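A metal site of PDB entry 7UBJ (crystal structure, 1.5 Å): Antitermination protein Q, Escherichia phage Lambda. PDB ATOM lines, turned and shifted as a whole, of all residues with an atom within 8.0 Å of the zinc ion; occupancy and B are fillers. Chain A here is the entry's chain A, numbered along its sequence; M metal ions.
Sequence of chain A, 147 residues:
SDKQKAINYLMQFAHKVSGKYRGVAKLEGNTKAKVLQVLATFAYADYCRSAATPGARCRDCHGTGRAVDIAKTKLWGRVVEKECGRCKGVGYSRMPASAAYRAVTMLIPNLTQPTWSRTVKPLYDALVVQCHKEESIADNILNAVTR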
ATOM      1  N   ARG A  57      14.854 -25.381  13.099  1.00  0.00           N
ATOM      2  CA  ARG A  57      13.925 -24.784  12.152  1.00  0.00           C
ATOM      3  C   ARG A  57      12.584 -24.736  12.870  1.00  0.00           C
ATOM      4  O   ARG A  57      12.381 -25.404  13.875  1.00  0.00           O
ATOM      5  CB  ARG A  57      13.840 -25.555  10.832  1.00  0.00           C
ATOM      6  CG  ARG A  57      13.211 -26.890  10.946  1.00  0.00           C
ATOM      7  CD  ARG A  57      13.129 -27.578   9.607  1.00  0.00           C
ATOM      8  NE  ARG A  57      12.502 -28.880   9.761  1.00  0.00           N
ATOM      9  CZ  ARG A  57      12.302 -29.750   8.781  1.00  0.00           C
ATOM     10  NH1 ARG A  57      12.662 -29.449   7.520  1.00  0.00           N
ATOM     11  NH2 ARG A  57      11.745 -30.909   9.064  1.00  0.00           N
ATOM     12  N   CYS A  58      11.700 -23.903  12.345  1.00  0.00           N
ATOM     13  CA  CYS A  58      10.379 -23.732  12.960  1.00  0.00           C
ATOM     14  C   CYS A  58       9.592 -25.016  13.023  1.00  0.00           C
ATOM     15  O   CYS A  58       9.500 -25.780  12.042  1.00  0.00           O
ATOM     16  CB  CYS A  58       9.596 -22.689  12.156  1.00  0.00           C
ATOM     17  SG  CYS A  58       7.885 -22.451  12.761  1.00  0.00           S
ATOM     18  N   ARG A  59       8.973 -25.249  14.177  1.00  0.00           N
ATOM     19  CA  ARG A  59       8.278 -26.509  14.440  1.00  0.00           C
ATOM     20  C   ARG A  59       6.856 -26.548  13.882  1.00  0.00           C
ATOM     21  O   ARG A  59       6.269 -27.634  13.837  1.00  0.00           O
ATOM     22  CB  ARG A  59       8.294 -26.827  15.939  1.00  0.00           C
ATOM     23  CG  ARG A  59       7.945 -25.658  16.851  1.00  0.00           C
ATOM     24  CD  ARG A  59       9.083 -25.371  17.846  1.00  0.00           C
ATOM     25  NE  ARG A  59       9.803 -24.110  17.640  1.00  0.00           N
ATOM     26  CZ  ARG A  59      10.986 -23.996  17.035  1.00  0.00           C
ATOM     27  NH1 ARG A  59      11.602 -25.064  16.542  1.00  0.00           N
ATOM     28  NH2 ARG A  59      11.564 -22.801  16.919  1.00  0.00           N
ATOM     29  N   ASP A  60       6.304 -25.421  13.415  1.00  0.00           N
ATOM     30  CA  ASP A  60       4.975 -25.427  12.813  1.00  0.00           C
ATOM     31  C   ASP A  60       5.030 -25.597  11.300  1.00  0.00           C
ATOM     32  O   ASP A  60       4.263 -26.390  10.734  1.00  0.00           O
ATOM     33  CB  ASP A  60       4.238 -24.128  13.140  1.00  0.00           C
ATOM     34  CG  ASP A  60       3.654 -24.126  14.525  1.00  0.00           C
ATOM     35  OD1 ASP A  60       3.939 -25.078  15.284  1.00  0.00           O
ATOM     36  OD2 ASP A  60       2.909 -23.171  14.862  1.00  0.00           O
ATOM     37  N   CYS A  61       5.909 -24.863  10.643  1.00  0.00           N
ATOM     38  CA  CYS A  61       6.039 -24.922   9.197  1.00  0.00           C
ATOM     39  C   CYS A  61       7.171 -25.817   8.740  1.00  0.00           C
ATOM     40  O   CYS A  61       7.320 -26.057   7.532  1.00  0.00           O
ATOM     41  CB  CYS A  61       6.242 -23.518   8.639  1.00  0.00           C
ATOM     42  SG  CYS A  61       7.765 -22.732   9.101  1.00  0.00           S
ATOM     43  N   HIS A  62       7.991 -26.315   9.661  1.00  0.00           N
ATOM     44  CA  HIS A  62       9.119 -27.173   9.296  1.00  0.00           C
ATOM     45  C   HIS A  62      10.010 -26.524   8.237  1.00  0.00           C
ATOM     46  O   HIS A  62      10.529 -27.182   7.341  1.00  0.00           O
ATOM     47  CB  HIS A  62       8.645 -28.572   8.919  1.00  0.00           C
ATOM     48  CG  HIS A  62       7.770 -29.201   9.944  1.00  0.00           C
ATOM     49  ND1 HIS A  62       8.248 -29.656  11.159  1.00  0.00           N
ATOM     50  CD2 HIS A  62       6.431 -29.436   9.956  1.00  0.00           C
ATOM     51  CE1 HIS A  62       7.238 -30.162  11.865  1.00  0.00           C
ATOM     52  NE2 HIS A  62       6.134 -30.061  11.149  1.00  0.00           N
ATOM     53  N   GLY A  63      10.246 -25.217   8.393  1.00  0.00           N
ATOM     54  CA  GLY A  63      11.234 -24.515   7.607  1.00  0.00           C
ATOM     55  C   GLY A  63      10.724 -23.723   6.431  1.00  0.00           C
ATOM     56  O   GLY A  63      11.464 -22.922   5.874  1.00  0.00           O
ATOM     57  N   THR A  64       9.485 -23.949   6.005  1.00  0.00           N
ATOM     58  CA  THR A  64       9.041 -23.281   4.785  1.00  0.00           C
ATOM     59  C   THR A  64       8.705 -21.814   4.992  1.00  0.00           C
ATOM     60  O   THR A  64       8.647 -21.067   4.009  1.00  0.00           O
ATOM     61  CB  THR A  64       7.789 -23.962   4.228  1.00  0.00           C
ATOM     62  OG1 THR A  64       6.696 -23.714   5.104  1.00  0.00           O
ATOM     63  CG2 THR A  64       7.983 -25.434   4.031  1.00  0.00           C
ATOM     64  N   GLY A  65       8.454 -21.393   6.235  1.00  0.00           N
ATOM     65  CA  GLY A  65       7.954 -20.059   6.525  1.00  0.00           C
ATOM     66  C   GLY A  65       6.492 -19.851   6.187  1.00  0.00           C
ATOM     67  O   GLY A  65       5.989 -18.737   6.368  1.00  0.00           O
ATOM     68  N   ARG A  66       5.802 -20.863   5.675  1.00  0.00           N
ATOM     69  CA  ARG A  66       4.449 -20.667   5.158  1.00  0.00           C
ATOM     70  C   ARG A  66       3.476 -21.645   5.810  1.00  0.00           C
ATOM     71  O   ARG A  66       3.864 -22.703   6.303  1.00  0.00           O
ATOM     72  CB  ARG A  66       4.386 -20.862   3.628  1.00  0.00           C
ATOM     73  CG  ARG A  66       5.463 -20.101   2.849  1.00  0.00           C
ATOM     74  CD  ARG A  66       5.232 -18.603   2.830  1.00  0.00           C
ATOM     75  NE  ARG A  66       4.167 -18.253   1.891  1.00  0.00           N
ATOM     76  CZ  ARG A  66       3.504 -17.105   1.902  1.00  0.00           C
ATOM     77  NH1 ARG A  66       3.775 -16.177   2.808  1.00  0.00           N
ATOM     78  NH2 ARG A  66       2.542 -16.892   1.008  1.00  0.00           N
ATOM     79  N   ALA A  67       2.192 -21.286   5.763  1.00  0.00           N
ATOM     80  CA  ALA A  67       1.112 -22.147   6.203  1.00  0.00           C
ATOM     81  C   ALA A  67      -0.008 -22.077   5.175  1.00  0.00           C
ATOM     82  O   ALA A  67      -0.052 -21.142   4.367  1.00  0.00           O
ATOM     83  CB  ALA A  67       0.561 -21.711   7.564  1.00  0.00           C
ATOM     84  N   GLU A  83       1.713 -16.398   5.547  1.00  0.00           N
ATOM     85  CA  GLU A  83       2.877 -16.438   6.418  1.00  0.00           C
ATOM     86  C   GLU A  83       2.645 -17.382   7.590  1.00  0.00           C
ATOM     87  O   GLU A  83       1.543 -17.445   8.148  1.00  0.00           O
ATOM     88  CB  GLU A  83       3.183 -15.033   6.943  1.00  0.00           C
ATOM     89  CG  GLU A  83       4.426 -14.933   7.802  1.00  0.00           C
ATOM     90  CD  GLU A  83       4.795 -13.493   8.128  1.00  0.00           C
ATOM     91  OE1 GLU A  83       5.306 -12.784   7.239  1.00  0.00           O
ATOM     92  OE2 GLU A  83       4.568 -13.065   9.289  1.00  0.00           O
ATOM     93  N   CYS A  84       3.686 -18.133   7.962  1.00  0.00           N
ATOM     94  CA  CYS A  84       3.652 -18.939   9.177  1.00  0.00           C
ATOM     95  C   CYS A  84       3.661 -18.003  10.383  1.00  0.00           C
ATOM     96  O   CYS A  84       4.597 -17.213  10.546  1.00  0.00           O
ATOM     97  CB  CYS A  84       4.855 -19.881   9.251  1.00  0.00           C
ATOM     98  SG  CYS A  84       4.996 -20.857  10.829  1.00  0.00           S
ATOM     99  N   GLY A  85       2.643 -18.123  11.231  1.00  0.00           N
ATOM    100  CA  GLY A  85       2.518 -17.186  12.349  1.00  0.00           C
ATOM    101  C   GLY A  85       3.602 -17.358  13.396  1.00  0.00           C
ATOM    102  O   GLY A  85       4.060 -16.387  13.996  1.00  0.00           O
ATOM    103  N   ARG A  86       4.031 -18.606  13.624  1.00  0.00           N
ATOM    104  CA  ARG A  86       4.989 -18.865  14.693  1.00  0.00           C
ATOM    105  C   ARG A  86       6.327 -18.204  14.395  1.00  0.00           C
ATOM    106  O   ARG A  86       6.856 -17.453  15.225  1.00  0.00           O
ATOM    107  CB  ARG A  86       5.143 -20.359  14.928  1.00  0.00           C
ATOM    108  CG  ARG A  86       6.134 -20.693  16.038  1.00  0.00           C
ATOM    109  CD  ARG A  86       6.167 -22.181  16.335  1.00  0.00           C
ATOM    110  NE  ARG A  86       7.109 -22.496  17.416  1.00  0.00           N
ATOM    111  CZ  ARG A  86       6.799 -22.511  18.715  1.00  0.00           C
ATOM    112  NH1 ARG A  86       5.560 -22.227  19.116  1.00  0.00           N
ATOM    113  NH2 ARG A  86       7.729 -22.811  19.612  1.00  0.00           N
ATOM    114  N   CYS A  87       6.920 -18.478  13.232  1.00  0.00           N
ATOM    115  CA  CYS A  87       8.218 -17.912  12.903  1.00  0.00           C
ATOM    116  C   CYS A  87       8.134 -16.605  12.114  1.00  0.00           C
ATOM    117  O   CYS A  87       9.181 -16.056  11.754  1.00  0.00           O
ATOM    118  CB  CYS A  87       9.073 -18.913  12.108  1.00  0.00           C
ATOM    119  SG  CYS A  87       8.367 -19.307  10.484  1.00  0.00           S
ATOM    120  N   LYS A  88       6.920 -16.108  11.864  1.00  0.00           N
ATOM    121  CA  LYS A  88       6.681 -14.944  11.005  1.00  0.00           C
ATOM    122  C   LYS A  88       7.533 -15.026   9.741  1.00  0.00           C
ATOM    123  O   LYS A  88       8.148 -14.053   9.303  1.00  0.00           O
ATOM    124  CB  LYS A  88       6.847 -13.612  11.758  1.00  0.00           C
ATOM    125  CG  LYS A  88       7.975 -13.555  12.761  1.00  0.00           C
ATOM    126  CD  LYS A  88       7.596 -12.691  13.981  1.00  0.00           C
ATOM    127  CE  LYS A  88       7.604 -11.194  13.682  1.00  0.00           C
ATOM    128  NZ  LYS A  88       7.382 -10.385  14.924  1.00  0.00           N
ATOM    129  N   GLY A  89       7.578 -16.221   9.152  1.00  0.00           N
ATOM    130  CA  GLY A  89       8.147 -16.414   7.849  1.00  0.00           C
ATOM    131  C   GLY A  89       9.635 -16.674   7.776  1.00  0.00           C
ATOM    132  O   GLY A  89      10.149 -16.867   6.670  1.00  0.00           O
ATOM    133  N   VAL A  90      10.357 -16.715   8.902  1.00  0.00           N
ATOM    134  CA  VAL A  90      11.795 -16.942   8.825  1.00  0.00           C
ATOM    135  C   VAL A  90      12.100 -18.393   8.489  1.00  0.00           C
ATOM    136  O   VAL A  90      12.996 -18.685   7.680  1.00  0.00           O
ATOM    137  CB  VAL A  90      12.508 -16.455  10.098  1.00  0.00           C
ATOM    138  CG1 VAL A  90      14.007 -16.731  10.011  1.00  0.00           C
ATOM    139  CG2 VAL A  90      12.266 -14.970  10.254  1.00  0.00           C
ATOM    140  N   GLY A  91      11.367 -19.320   9.087  1.00  0.00           N
ATOM    141  CA  GLY A  91      11.519 -20.744   8.847  1.00  0.00           C
ATOM    142  C   GLY A  91      12.720 -21.443   9.441  1.00  0.00           C
ATOM    143  O   GLY A  91      12.573 -22.512  10.060  1.00  0.00           O
ATOM    144  N   TYR A  92      13.911 -20.891   9.240  1.00  0.00           N
ATOM    145  CA  TYR A  92      15.152 -21.565   9.584  1.00  0.00           C
ATOM    146  C   TYR A  92      16.218 -20.527   9.913  1.00  0.00           C
ATOM    147  O   TYR A  92      16.178 -19.400   9.420  1.00  0.00           O
ATOM    148  CB  TYR A  92      15.635 -22.463   8.427  1.00  0.00           C
ATOM    149  CG  TYR A  92      15.826 -21.702   7.125  1.00  0.00           C
ATOM    150  CD1 TYR A  92      17.055 -21.144   6.811  1.00  0.00           C
ATOM    151  CD2 TYR A  92      14.774 -21.541   6.237  1.00  0.00           C
ATOM    152  CE1 TYR A  92      17.245 -20.448   5.646  1.00  0.00           C
ATOM    153  CE2 TYR A  92      14.951 -20.818   5.065  1.00  0.00           C
ATOM    154  CZ  TYR A  92      16.191 -20.275   4.784  1.00  0.00           C
ATOM    155  OH  TYR A  92      16.350 -19.574   3.599  1.00  0.00           O
HETATM  156 ZN    ZN M   1       7.149 -21.342  10.824  1.00  0.00          ZN
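Within 4 Å of the zinc ion: Cys 58, Cys 61, Cys 84 and Cys 87.
The backbone NH of Arg 86 sits close to the side-chain sulfur of Cys 84 (3.7 Å). The backbone carbonyl oxygen (O) of Cys 84 lies within hydrogen-bond range of the backbone NH (N) of Gly 89 (3.4 Å). The side-chain sulfur (SG) of Cys 61 lies close to the backbone NH (N) of Gly 65, 3.2 Å away. OG1 of Thr 64 lies within hydrogen-bond range of O of Cys 61 (3.4 Å). The backbone NH (N) of Asp 60 sits close to the side-chain sulfur (SG) of Cys 58, 3.4 Å away. The backbone NH of Cys 58 is in hydrogen-bond range of the backbone carbonyl oxygen of Gly 91, 2.8 Å away. N of Gly 91 lies close to SG of Cys 87 (3.3 Å). N of Val 90 lies close to SG of Cys 87.
SG of Cys 84 is bound to the zinc ion (2.2 Å). The zinc ion is bound by SG of Cys 61, at 2.3 Å. The zinc ion is bound by the side-chain sulfur (SG) of Cys 58, 2.4 Å away. The zinc ion is bound by SG of Cys 87 (2.4 Å). The zinc ion has four donor atoms within binding distance.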
